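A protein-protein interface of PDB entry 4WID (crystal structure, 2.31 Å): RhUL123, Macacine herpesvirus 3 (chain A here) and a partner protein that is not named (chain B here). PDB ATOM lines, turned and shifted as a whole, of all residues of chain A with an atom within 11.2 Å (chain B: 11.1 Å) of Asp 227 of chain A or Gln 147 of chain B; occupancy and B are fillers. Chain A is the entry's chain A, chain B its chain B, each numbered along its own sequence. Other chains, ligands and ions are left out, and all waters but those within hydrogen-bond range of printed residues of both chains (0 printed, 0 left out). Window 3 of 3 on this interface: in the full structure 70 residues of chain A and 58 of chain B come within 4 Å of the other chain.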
ATOM      1  N   VAL A  63     -19.895  -4.342  25.652  1.00  0.00           N
ATOM      2  CA  VAL A  63     -20.065  -4.148  24.226  1.00  0.00           C
ATOM      3  C   VAL A  63     -19.853  -2.671  23.834  1.00  0.00           C
ATOM      4  O   VAL A  63     -19.572  -2.357  22.677  1.00  0.00           O
ATOM      5  CB  VAL A  63     -21.468  -4.640  23.790  1.00  0.00           C
ATOM      6  CG1 VAL A  63     -22.552  -3.765  24.401  1.00  0.00           C
ATOM      7  CG2 VAL A  63     -21.590  -4.693  22.273  1.00  0.00           C
ATOM      8  N   HIS A  67     -16.449  -1.133  21.831  1.00  0.00           N
ATOM      9  CA  HIS A  67     -16.651  -0.275  20.678  1.00  0.00           C
ATOM     10  C   HIS A  67     -15.736   0.947  20.695  1.00  0.00           C
ATOM     11  O   HIS A  67     -15.135   1.305  19.676  1.00  0.00           O
ATOM     12  CB  HIS A  67     -18.105   0.175  20.597  1.00  0.00           C
ATOM     13  CG  HIS A  67     -18.448   0.843  19.306  1.00  0.00           C
ATOM     14  ND1 HIS A  67     -18.132   0.295  18.081  1.00  0.00           N
ATOM     15  CD2 HIS A  67     -19.066   2.018  19.046  1.00  0.00           C
ATOM     16  CE1 HIS A  67     -18.548   1.102  17.121  1.00  0.00           C
ATOM     17  NE2 HIS A  67     -19.118   2.155  17.678  1.00  0.00           N
ATOM     18  N   PHE A 219     -16.221   1.913   6.834  1.00  0.00           N
ATOM     19  CA  PHE A 219     -16.671   1.459   8.141  1.00  0.00           C
ATOM     20  C   PHE A 219     -17.179   2.619   8.984  1.00  0.00           C
ATOM     21  O   PHE A 219     -18.288   2.581   9.524  1.00  0.00           O
ATOM     22  CB  PHE A 219     -15.534   0.752   8.876  1.00  0.00           C
ATOM     23  CG  PHE A 219     -15.902   0.260  10.260  1.00  0.00           C
ATOM     24  CD1 PHE A 219     -16.736  -0.832  10.426  1.00  0.00           C
ATOM     25  CD2 PHE A 219     -15.379   0.873  11.389  1.00  0.00           C
ATOM     26  CE1 PHE A 219     -17.049  -1.293  11.689  1.00  0.00           C
ATOM     27  CE2 PHE A 219     -15.695   0.422  12.652  1.00  0.00           C
ATOM     28  CZ  PHE A 219     -16.529  -0.662  12.804  1.00  0.00           C
ATOM     29  N   MLZ A 221     -18.093   5.446   8.055  1.00  0.00           N
ATOM     30  CA  MLZ A 221     -19.237   6.094   7.431  1.00  0.00           C
ATOM     31  CB  MLZ A 221     -19.229   5.920   5.915  1.00  0.00           C
ATOM     32  CG  MLZ A 221     -18.467   7.039   5.220  1.00  0.00           C
ATOM     33  CD  MLZ A 221     -19.028   7.337   3.830  1.00  0.00           C
ATOM     34  CE  MLZ A 221     -18.090   8.280   3.083  1.00  0.00           C
ATOM     35  NZ  MLZ A 221     -18.442   8.467   1.686  1.00  0.00           N
ATOM     36  CM  MLZ A 221     -18.291   7.379   0.739  1.00  0.00           C
ATOM     37  C   MLZ A 221     -20.503   5.467   7.935  1.00  0.00           C
ATOM     38  O   MLZ A 221     -21.437   6.190   8.355  1.00  0.00           O
ATOM     39  N   GLN A 222     -20.563   4.140   7.911  1.00  0.00           N
ATOM     40  CA  GLN A 222     -21.805   3.420   8.188  1.00  0.00           C
ATOM     41  C   GLN A 222     -21.965   3.025   9.656  1.00  0.00           C
ATOM     42  O   GLN A 222     -22.705   2.093   9.976  1.00  0.00           O
ATOM     43  CB  GLN A 222     -21.878   2.167   7.321  1.00  0.00           C
ATOM     44  CG  GLN A 222     -21.336   2.356   5.934  1.00  0.00           C
ATOM     45  CD  GLN A 222     -20.914   1.044   5.314  1.00  0.00           C
ATOM     46  OE1 GLN A 222     -21.749   0.289   4.815  1.00  0.00           O
ATOM     47  NE2 GLN A 222     -19.609   0.759   5.347  1.00  0.00           N
ATOM     48  N   LEU A 223     -21.271   3.734  10.538  1.00  0.00           N
ATOM     49  CA  LEU A 223     -21.260   3.398  11.953  1.00  0.00           C
ATOM     50  C   LEU A 223     -22.659   3.595  12.557  1.00  0.00           C
ATOM     51  O   LEU A 223     -23.086   2.833  13.427  1.00  0.00           O
ATOM     52  CB  LEU A 223     -20.207   4.247  12.679  1.00  0.00           C
ATOM     53  CG  LEU A 223     -19.425   3.688  13.871  1.00  0.00           C
ATOM     54  CD1 LEU A 223     -19.118   2.207  13.701  1.00  0.00           C
ATOM     55  CD2 LEU A 223     -18.133   4.483  14.049  1.00  0.00           C
ATOM     56  N   SER A 224     -23.381   4.600  12.068  1.00  0.00           N
ATOM     57  CA  SER A 224     -24.748   4.846  12.522  1.00  0.00           C
ATOM     58  C   SER A 224     -25.724   3.766  12.035  1.00  0.00           C
ATOM     59  O   SER A 224     -26.651   3.401  12.762  1.00  0.00           O
ATOM     60  CB  SER A 224     -25.227   6.228  12.066  1.00  0.00           C
ATOM     61  OG  SER A 224     -25.123   6.370  10.661  1.00  0.00           O
ATOM     62  N   ASN A 225     -25.505   3.244  10.824  1.00  0.00           N
ATOM     63  CA  ASN A 225     -26.399   2.236  10.246  1.00  0.00           C
ATOM     64  C   ASN A 225     -26.231   0.824  10.816  1.00  0.00           C
ATOM     65  O   ASN A 225     -26.713  -0.141  10.224  1.00  0.00           O
ATOM     66  CB  ASN A 225     -26.220   2.161   8.731  1.00  0.00           C
ATOM     67  CG  ASN A 225     -26.472   3.484   8.036  1.00  0.00           C
ATOM     68  OD1 ASN A 225     -25.560   4.296   7.872  1.00  0.00           O
ATOM     69  ND2 ASN A 225     -27.708   3.693   7.596  1.00  0.00           N
ATOM     70  N   TYR A 226     -25.538   0.698  11.943  1.00  0.00           N
ATOM     71  CA  TYR A 226     -25.406  -0.590  12.618  1.00  0.00           C
ATOM     72  C   TYR A 226     -26.405  -0.704  13.776  1.00  0.00           C
ATOM     73  O   TYR A 226     -26.210  -0.094  14.829  1.00  0.00           O
ATOM     74  CB  TYR A 226     -23.985  -0.786  13.154  1.00  0.00           C
ATOM     75  CG  TYR A 226     -22.944  -1.266  12.157  1.00  0.00           C
ATOM     76  CD1 TYR A 226     -22.903  -2.594  11.745  1.00  0.00           C
ATOM     77  CD2 TYR A 226     -21.968  -0.399  11.669  1.00  0.00           C
ATOM     78  CE1 TYR A 226     -21.937  -3.038  10.846  1.00  0.00           C
ATOM     79  CE2 TYR A 226     -20.998  -0.834  10.773  1.00  0.00           C
ATOM     80  CZ  TYR A 226     -20.986  -2.156  10.366  1.00  0.00           C
ATOM     81  OH  TYR A 226     -20.023  -2.591   9.479  1.00  0.00           O
ATOM     82  N   ASP A 227     -27.463  -1.486  13.589  1.00  0.00           N
ATOM     83  CA  ASP A 227     -28.488  -1.632  14.626  1.00  0.00           C
ATOM     84  C   ASP A 227     -27.923  -2.302  15.877  1.00  0.00           C
ATOM     85  O   ASP A 227     -28.236  -1.913  17.001  1.00  0.00           O
ATOM     86  CB  ASP A 227     -29.681  -2.425  14.090  1.00  0.00           C
ATOM     87  CG  ASP A 227     -30.296  -1.783  12.864  1.00  0.00           C
ATOM     88  OD1 ASP A 227     -30.437  -0.541  12.852  1.00  0.00           O
ATOM     89  OD2 ASP A 227     -30.619  -2.513  11.904  1.00  0.00           O
ATOM     90  N   ASP A 228     -27.068  -3.297  15.661  1.00  0.00           N
ATOM     91  CA  ASP A 228     -26.458  -4.073  16.737  1.00  0.00           C
ATOM     92  C   ASP A 228     -24.975  -3.725  16.887  1.00  0.00           C
ATOM     93  O   ASP A 228     -24.182  -3.919  15.961  1.00  0.00           O
ATOM     94  CB  ASP A 228     -26.629  -5.571  16.458  1.00  0.00           C
ATOM     95  CG  ASP A 228     -26.412  -6.433  17.688  1.00  0.00           C
ATOM     96  OD1 ASP A 228     -25.770  -5.965  18.653  1.00  0.00           O
ATOM     97  OD2 ASP A 228     -26.884  -7.591  17.682  1.00  0.00           O
ATOM     98  N   LEU A 229     -24.597  -3.222  18.058  1.00  0.00           N
ATOM     99  CA  LEU A 229     -23.207  -2.852  18.296  1.00  0.00           C
ATOM    100  C   LEU A 229     -22.303  -4.076  18.416  1.00  0.00           C
ATOM    101  O   LEU A 229     -21.084  -3.941  18.352  1.00  0.00           O
ATOM    102  CB  LEU A 229     -23.074  -1.974  19.544  1.00  0.00           C
ATOM    103  CG  LEU A 229     -23.223  -0.467  19.293  1.00  0.00           C
ATOM    104  CD1 LEU A 229     -24.684  -0.021  19.397  1.00  0.00           C
ATOM    105  CD2 LEU A 229     -22.324   0.353  20.223  1.00  0.00           C
ATOM    106  N   THR A 230     -22.879  -5.266  18.577  1.00  0.00           N
ATOM    107  CA  THR A 230     -22.056  -6.476  18.531  1.00  0.00           C
ATOM    108  C   THR A 230     -21.631  -6.776  17.086  1.00  0.00           C
ATOM    109  O   THR A 230     -20.601  -7.414  16.856  1.00  0.00           O
ATOM    110  CB  THR A 230     -22.777  -7.711  19.119  1.00  0.00           C
ATOM    111  OG1 THR A 230     -23.888  -8.067  18.293  1.00  0.00           O
ATOM    112  CG2 THR A 230     -23.258  -7.431  20.533  1.00  0.00           C
ATOM    113  N   ASP A 231     -22.430  -6.313  16.127  1.00  0.00           N
ATOM    114  CA  ASP A 231     -22.102  -6.447  14.716  1.00  0.00           C
ATOM    115  C   ASP A 231     -21.028  -5.450  14.320  1.00  0.00           C
ATOM    116  O   ASP A 231     -20.035  -5.807  13.696  1.00  0.00           O
ATOM    117  CB  ASP A 231     -23.331  -6.226  13.839  1.00  0.00           C
ATOM    118  CG  ASP A 231     -24.335  -7.336  13.954  1.00  0.00           C
ATOM    119  OD1 ASP A 231     -24.024  -8.356  14.608  1.00  0.00           O
ATOM    120  OD2 ASP A 231     -25.429  -7.183  13.372  1.00  0.00           O
ATOM    121  N   ALA A 232     -21.266  -4.191  14.675  1.00  0.00           N
ATOM    122  CA  ALA A 232     -20.323  -3.119  14.421  1.00  0.00           C
ATOM    123  C   ALA A 232     -18.971  -3.427  15.062  1.00  0.00           C
ATOM    124  O   ALA A 232     -17.922  -3.181  14.463  1.00  0.00           O
ATOM    125  CB  ALA A 232     -20.872  -1.802  14.937  1.00  0.00           C
ATOM    126  N   ASN A 233     -18.993  -3.972  16.274  1.00  0.00           N
ATOM    127  CA  ASN A 233     -17.754  -4.382  16.922  1.00  0.00           C
ATOM    128  C   ASN A 233     -17.078  -5.501  16.149  1.00  0.00           C
ATOM    129  O   ASN A 233     -15.853  -5.534  16.059  1.00  0.00           O
ATOM    130  CB  ASN A 233     -17.998  -4.832  18.367  1.00  0.00           C
ATOM    131  CG  ASN A 233     -18.228  -3.669  19.308  1.00  0.00           C
ATOM    132  OD1 ASN A 233     -17.923  -2.523  18.976  1.00  0.00           O
ATOM    133  ND2 ASN A 233     -18.778  -3.956  20.494  1.00  0.00           N
ATOM    134  N   HIS A 234     -17.879  -6.412  15.598  1.00  0.00           N
ATOM    135  CA  HIS A 234     -17.338  -7.569  14.892  1.00  0.00           C
ATOM    136  C   HIS A 234     -16.572  -7.132  13.632  1.00  0.00           C
ATOM    137  O   HIS A 234     -15.406  -7.512  13.445  1.00  0.00           O
ATOM    138  CB  HIS A 234     -18.445  -8.566  14.524  1.00  0.00           C
ATOM    139  CG  HIS A 234     -17.934  -9.793  13.832  1.00  0.00           C
ATOM    140  ND1 HIS A 234     -17.680  -9.833  12.477  1.00  0.00           N
ATOM    141  CD2 HIS A 234     -17.592 -11.012  14.314  1.00  0.00           C
ATOM    142  CE1 HIS A 234     -17.214 -11.027  12.151  1.00  0.00           C
ATOM    143  NE2 HIS A 234     -17.148 -11.760  13.247  1.00  0.00           N
ATOM    144  N   ASP A 235     -17.225  -6.337  12.783  1.00  0.00           N
ATOM    145  CA  ASP A 235     -16.572  -5.805  11.584  1.00  0.00           C
ATOM    146  C   ASP A 235     -15.329  -4.997  11.958  1.00  0.00           C
ATOM    147  O   ASP A 235     -14.290  -5.142  11.335  1.00  0.00           O
ATOM    148  CB  ASP A 235     -17.543  -4.942  10.764  1.00  0.00           C
ATOM    149  CG  ASP A 235     -18.596  -5.768  10.029  1.00  0.00           C
ATOM    150  OD1 ASP A 235     -18.493  -7.013  10.028  1.00  0.00           O
ATOM    151  OD2 ASP A 235     -19.514  -5.164   9.428  1.00  0.00           O
ATOM    152  N   THR B 142     -14.766  -5.476   2.457  1.00  0.00           N
ATOM    153  CA  THR B 142     -15.470  -4.231   2.740  1.00  0.00           C
ATOM    154  C   THR B 142     -16.508  -4.453   3.847  1.00  0.00           C
ATOM    155  O   THR B 142     -17.366  -5.326   3.731  1.00  0.00           O
ATOM    156  CB  THR B 142     -16.155  -3.656   1.477  1.00  0.00           C
ATOM    157  OG1 THR B 142     -15.150  -3.240   0.537  1.00  0.00           O
ATOM    158  CG2 THR B 142     -17.013  -2.466   1.835  1.00  0.00           C
ATOM    159  N   PRO B 143     -16.407  -3.668   4.935  1.00  0.00           N
ATOM    160  CA  PRO B 143     -17.356  -3.696   6.049  1.00  0.00           C
ATOM    161  C   PRO B 143     -18.679  -3.053   5.675  1.00  0.00           C
ATOM    162  O   PRO B 143     -18.706  -1.984   5.057  1.00  0.00           O
ATOM    163  CB  PRO B 143     -16.646  -2.884   7.134  1.00  0.00           C
ATOM    164  CG  PRO B 143     -15.778  -1.944   6.373  1.00  0.00           C
ATOM    165  CD  PRO B 143     -15.295  -2.731   5.188  1.00  0.00           C
ATOM    166  N   VAL B 144     -19.773  -3.707   6.042  1.00  0.00           N
ATOM    167  CA  VAL B 144     -21.097  -3.200   5.718  1.00  0.00           C
ATOM    168  C   VAL B 144     -22.107  -3.808   6.683  1.00  0.00           C
ATOM    169  O   VAL B 144     -22.023  -4.999   7.008  1.00  0.00           O
ATOM    170  CB  VAL B 144     -21.480  -3.511   4.237  1.00  0.00           C
ATOM    171  CG1 VAL B 144     -21.470  -5.004   3.973  1.00  0.00           C
ATOM    172  CG2 VAL B 144     -22.829  -2.910   3.873  1.00  0.00           C
ATOM    173  N   PRO B 145     -23.031  -2.978   7.192  1.00  0.00           N
ATOM    174  CA  PRO B 145     -24.095  -3.496   8.055  1.00  0.00           C
ATOM    175  C   PRO B 145     -24.798  -4.671   7.381  1.00  0.00           C
ATOM    176  O   PRO B 145     -25.033  -4.617   6.174  1.00  0.00           O
ATOM    177  CB  PRO B 145     -25.026  -2.295   8.220  1.00  0.00           C
ATOM    178  CG  PRO B 145     -24.113  -1.113   8.096  1.00  0.00           C
ATOM    179  CD  PRO B 145     -23.079  -1.508   7.075  1.00  0.00           C
ATOM    180  N   PRO B 146     -25.090  -5.736   8.143  1.00  0.00           N
ATOM    181  CA  PRO B 146     -25.693  -6.965   7.612  1.00  0.00           C
ATOM    182  C   PRO B 146     -27.064  -6.738   6.976  1.00  0.00           C
ATOM    183  O   PRO B 146     -27.464  -7.534   6.127  1.00  0.00           O
ATOM    184  CB  PRO B 146     -25.812  -7.863   8.852  1.00  0.00           C
ATOM    185  CG  PRO B 146     -25.795  -6.920  10.009  1.00  0.00           C
ATOM    186  CD  PRO B 146     -24.873  -5.814   9.597  1.00  0.00           C
ATOM    187  N   GLN B 147     -27.764  -5.676   7.376  1.00  0.00           N
ATOM    188  CA  GLN B 147     -29.061  -5.353   6.786  1.00  0.00           C
ATOM    189  C   GLN B 147     -28.916  -4.583   5.477  1.00  0.00           C
ATOM    190  O   GLN B 147     -29.917  -4.253   4.842  1.00  0.00           O
ATOM    191  CB  GLN B 147     -29.917  -4.542   7.758  1.00  0.00           C
ATOM    192  CG  GLN B 147     -29.549  -3.067   7.849  1.00  0.00           C
ATOM    193  CD  GLN B 147     -28.444  -2.795   8.854  1.00  0.00           C
ATOM    194  OE1 GLN B 147     -27.788  -3.717   9.340  1.00  0.00           O
ATOM    195  NE2 GLN B 147     -28.238  -1.524   9.176  1.00  0.00           N
ATOM    196  N   TYR B 148     -27.675  -4.286   5.088  1.00  0.00           N
ATOM    197  CA  TYR B 148     -27.390  -3.664   3.793  1.00  0.00           C
ATOM    198  C   TYR B 148     -26.464  -4.528   2.935  1.00  0.00           C
ATOM    199  O   TYR B 148     -26.221  -4.200   1.773  1.00  0.00           O
ATOM    200  CB  TYR B 148     -26.761  -2.277   3.967  1.00  0.00           C
ATOM    201  CG  TYR B 148     -27.678  -1.250   4.578  1.00  0.00           C
ATOM    202  CD1 TYR B 148     -28.755  -0.735   3.861  1.00  0.00           C
ATOM    203  CD2 TYR B 148     -27.469  -0.787   5.873  1.00  0.00           C
ATOM    204  CE1 TYR B 148     -29.602   0.211   4.424  1.00  0.00           C
ATOM    205  CE2 TYR B 148     -28.307   0.156   6.445  1.00  0.00           C
ATOM    206  CZ  TYR B 148     -29.370   0.653   5.717  1.00  0.00           C
ATOM    207  OH  TYR B 148     -30.201   1.591   6.288  1.00  0.00           O
ATOM    208  N   MLY B 149     -25.954  -5.621   3.509  1.00  0.00           N
ATOM    209  CA  MLY B 149     -25.004  -6.516   2.832  1.00  0.00           C
ATOM    210  CB  MLY B 149     -24.665  -7.707   3.738  1.00  0.00           C
ATOM    211  CG  MLY B 149     -23.693  -8.730   3.132  1.00  0.00           C
ATOM    212  CD  MLY B 149     -22.242  -8.265   3.237  1.00  0.00           C
ATOM    213  CE  MLY B 149     -21.270  -9.414   3.015  1.00  0.00           C
ATOM    214  NZ  MLY B 149     -19.813  -9.049   3.190  1.00  0.00           N
ATOM    215  CH1 MLY B 149     -18.982 -10.267   3.135  1.00  0.00           C
ATOM    216  CH2 MLY B 149     -19.357  -8.105   2.144  1.00  0.00           C
ATOM    217  C   MLY B 149     -25.550  -7.039   1.507  1.00  0.00           C
ATOM    218  O   MLY B 149     -24.817  -7.221   0.536  1.00  0.00           O
ATOM    219  N   GLU B 150     -26.850  -7.288   1.498  1.00  0.00           N
ATOM    220  CA  GLU B 150     -27.547  -7.782   0.324  1.00  0.00           C
ATOM    221  C   GLU B 150     -27.575  -6.739  -0.798  1.00  0.00           C
ATOM    222  O   GLU B 150     -27.349  -7.074  -1.954  1.00  0.00           O
ATOM    223  CB  GLU B 150     -28.979  -8.197   0.710  1.00  0.00           C
ATOM    224  CG  GLU B 150     -29.804  -8.788  -0.420  1.00  0.00           C
ATOM    225  CD  GLU B 150     -29.467 -10.244  -0.707  1.00  0.00           C
ATOM    226  OE1 GLU B 150     -28.281 -10.633  -0.587  1.00  0.00           O
ATOM    227  OE2 GLU B 150     -30.399 -11.003  -1.055  1.00  0.00           O
ATOM    228  N   LYS B 151     -27.867  -5.488  -0.433  1.00  0.00           N
ATOM    229  CA  LYS B 151     -27.974  -4.369  -1.367  1.00  0.00           C
ATOM    230  C   LYS B 151     -26.607  -4.072  -1.945  1.00  0.00           C
ATOM    231  O   LYS B 151     -26.488  -3.756  -3.132  1.00  0.00           O
ATOM    232  CB  LYS B 151     -28.548  -3.120  -0.670  1.00  0.00           C
ATOM    233  CG  LYS B 151     -28.882  -1.940  -1.596  1.00  0.00           C
ATOM    234  CD  LYS B 151     -29.680  -0.849  -0.855  1.00  0.00           C
ATOM    235  CE  LYS B 151     -30.428   0.100  -1.820  1.00  0.00           C
ATOM    236  NZ  LYS B 151     -31.917  -0.181  -2.018  1.00  0.00           N
ATOM    237  N   PHE B 152     -25.583  -4.188  -1.097  1.00  0.00           N
ATOM    238  CA  PHE B 152     -24.190  -4.016  -1.505  1.00  0.00           C
ATOM    239  C   PHE B 152     -23.786  -5.076  -2.532  1.00  0.00           C
ATOM    240  O   PHE B 152     -23.303  -4.735  -3.621  1.00  0.00           O
ATOM    241  CB  PHE B 152     -23.248  -4.070  -0.287  1.00  0.00           C
ATOM    242  CG  PHE B 152     -21.778  -3.873  -0.629  1.00  0.00           C
ATOM    243  CD1 PHE B 152     -21.359  -2.772  -1.361  1.00  0.00           C
ATOM    244  CD2 PHE B 152     -20.817  -4.777  -0.181  1.00  0.00           C
ATOM    245  CE1 PHE B 152     -20.012  -2.591  -1.664  1.00  0.00           C
ATOM    246  CE2 PHE B 152     -19.473  -4.605  -0.481  1.00  0.00           C
ATOM    247  CZ  PHE B 152     -19.066  -3.514  -1.220  1.00  0.00           C
ATOM    248  N   MET B 153     -24.004  -6.348  -2.188  1.00  0.00           N
ATOM    249  CA  MET B 153     -23.663  -7.447  -3.090  1.00  0.00           C
ATOM    250  C   MET B 153     -24.378  -7.342  -4.438  1.00  0.00           C
ATOM    251  O   MET B 153     -23.752  -7.505  -5.493  1.00  0.00           O
ATOM    252  CB  MET B 153     -23.998  -8.790  -2.455  1.00  0.00           C
ATOM    253  CG  MET B 153     -23.739  -9.966  -3.384  1.00  0.00           C
ATOM    254  SD  MET B 153     -24.355 -11.514  -2.702  1.00  0.00           S
ATOM    255  CE  MET B 153     -26.119 -11.211  -2.744  1.00  0.00           C
ATOM    256  N   VAL B 154     -25.688  -7.084  -4.401  1.00  0.00           N
ATOM    257  CA  VAL B 154     -26.462  -7.006  -5.634  1.00  0.00           C
ATOM    258  C   VAL B 154     -25.938  -5.910  -6.566  1.00  0.00           C
ATOM    259  O   VAL B 154     -25.733  -6.144  -7.747  1.00  0.00           O
ATOM    260  CB  VAL B 154     -27.953  -6.745  -5.364  1.00  0.00           C
ATOM    261  CG1 VAL B 154     -28.661  -6.377  -6.658  1.00  0.00           C
ATOM    262  CG2 VAL B 154     -28.620  -7.964  -4.699  1.00  0.00           C
ATOM    263  N   VAL B 306     -21.676   2.494  -1.514  1.00  0.00           N
ATOM    264  CA  VAL B 306     -21.872   2.695  -0.081  1.00  0.00           C
ATOM    265  C   VAL B 306     -22.365   4.107   0.221  1.00  0.00           C
ATOM    266  O   VAL B 306     -23.196   4.289   1.095  1.00  0.00           O
ATOM    267  CB  VAL B 306     -20.578   2.417   0.721  1.00  0.00           C
ATOM    268  CG1 VAL B 306     -20.779   2.751   2.201  1.00  0.00           C
ATOM    269  CG2 VAL B 306     -20.187   0.971   0.570  1.00  0.00           C
ATOM    270  N   ILE B 309     -25.943   4.231  -0.706  1.00  0.00           N
ATOM    271  CA  ILE B 309     -26.810   3.385   0.112  1.00  0.00           C
ATOM    272  C   ILE B 309     -26.991   3.948   1.516  1.00  0.00           C
ATOM    273  O   ILE B 309     -28.114   4.092   1.993  1.00  0.00           O
ATOM    274  CB  ILE B 309     -26.266   1.948   0.238  1.00  0.00           C
ATOM    275  CG1 ILE B 309     -26.334   1.219  -1.105  1.00  0.00           C
ATOM    276  CG2 ILE B 309     -27.053   1.163   1.289  1.00  0.00           C
ATOM    277  CD1 ILE B 309     -25.743  -0.169  -1.047  1.00  0.00           C
ATOM    278  N   HIS B 310     -25.871   4.242   2.172  1.00  0.00           N
ATOM    279  CA  HIS B 310     -25.844   4.782   3.531  1.00  0.00           C
ATOM    280  C   HIS B 310     -26.679   6.058   3.651  1.00  0.00           C
ATOM    281  O   HIS B 310     -27.386   6.258   4.644  1.00  0.00           O
ATOM    282  CB  HIS B 310     -24.389   5.033   3.949  1.00  0.00           C
ATOM    283  CG  HIS B 310     -24.225   6.053   5.034  1.00  0.00           C
ATOM    284  ND1 HIS B 310     -24.582   5.816   6.344  1.00  0.00           N
ATOM    285  CD2 HIS B 310     -23.719   7.308   5.003  1.00  0.00           C
ATOM    286  CE1 HIS B 310     -24.314   6.886   7.072  1.00  0.00           C
ATOM    287  NE2 HIS B 310     -23.791   7.806   6.282  1.00  0.00           N
ATOM    288  N   THR B 311     -26.596   6.910   2.630  1.00  0.00           N
ATOM    289  CA  THR B 311     -27.432   8.108   2.526  1.00  0.00           C
ATOM    290  C   THR B 311     -28.026   8.215   1.128  1.00  0.00           C
ATOM    291  O   THR B 311     -27.299   8.131   0.136  1.00  0.00           O
ATOM    292  CB  THR B 311     -26.637   9.403   2.831  1.00  0.00           C
ATOM    293  OG1 THR B 311     -25.416   9.416   2.073  1.00  0.00           O
ATOM    294  CG2 THR B 311     -26.321   9.513   4.322  1.00  0.00           C
ATOM    295  N   ASN B 317     -32.034  -0.014  -6.369  1.00  0.00           N
ATOM    296  CA  ASN B 317     -30.808  -0.556  -6.937  1.00  0.00           C
ATOM    297  C   ASN B 317     -30.614  -0.157  -8.393  1.00  0.00           C
ATOM    298  O   ASN B 317     -29.503   0.164  -8.819  1.00  0.00           O
ATOM    299  CB  ASN B 317     -30.796  -2.081  -6.811  1.00  0.00           C
ATOM    300  CG  ASN B 317     -30.741  -2.545  -5.360  1.00  0.00           C
ATOM    301  OD1 ASN B 317     -30.490  -1.751  -4.449  1.00  0.00           O
ATOM    302  ND2 ASN B 317     -30.970  -3.836  -5.143  1.00  0.00           N
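Among the printed residues, pairs that only touch across the chains: Gln 222 of chain A with Pro 145 of chain B, MLZ 221 of chain A with His 310 of chain B, Asn 225 of chain A with Pro 145 of chain B, Asp 231 of chain A with Pro 146 of chain B, Gln 222 of chain A with Val 144 of chain B, Asn 225 of chain A with Tyr 148 of chain B, Gln 222 of chain A with Val 306 of chain B, Tyr 226 of chain A with Pro 145 of chain B, Tyr 226 of chain A with Val 144 of chain B, Phe 219 of chain A with Pro 143 of chain B, Ser 224 of chain A with His 310 of chain B and Asp 227 of chain A with Gln 147 of chain B.
The backbone carbonyl oxygen of Val 144 of chain B lies close to the side-chain carboxylate of Asp 235 of chain A (3.5 Å). O of Asn 225 of chain A lies close to NE2 of Gln 147 of chain B, at 2.3 Å. O of Pro 143 of chain B lies within hydrogen-bond range of NE2 of Gln 222 of chain A. The side-chain amide oxygen (OD1) of Asn 225 of chain A sits close to a ring nitrogen (ND1) of His 310 of chain B (2.4 Å).
OD2 of Asp 235 of chain A sits at hydrogen-bond distance from OH of Tyr 226 of chain A (2.6 Å).
Printed residues of chain B within 4 Å of MLZ 221 of chain A: His 310. Of the printed residues of chain B, Gln 222 of chain A touches Pro 143, Val 144, Pro 145 and Val 306. Asn 225 of chain A touches just these residues of chain B: Pro 145 (3.4 Å), Gln 147 (2.3 Å), Tyr 148 (3.5 Å) and His 310 (2.4 Å). Asp 227 of chain A touches one residue of chain B. No residue of chain B comes within 4 Å of Asp 228 of chain A. Printed residues of chain B within 4 Å of Asp 231 of chain A: Pro 146. Of the printed residues of chain B, Asp 235 of chain A touches Val 144 (3.5 Å). Pro 145 of chain B touches just these residues of chain A: Gln 222, Asn 225 and Tyr 226. Pro 146 of chain B touches just one residue of chain A: Asp 231 (3.4 Å). Gln 147 of chain B touches just these residues of chain A: Asn 225 (2.3 Å) and Asp 227 (3.8 Å). Printed residues of chain A within 4 Å of Val 306 of chain B: Gln 222. The nearest residue of chain B that does not touch Asp 227 of chain A is Pro 145 of chain B (6.0 Å).
Hydrophobic or aromatic side chains of chain B within 4 Å of the printed part of chain A: Pro 143, Val 144, Pro 145, Pro 146, Tyr 148, Val 306 and His 310. Among the printed residues, no Asp or Glu carboxylate lies within 4 Å of a Lys or Arg side-chain nitrogen of the other chain.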
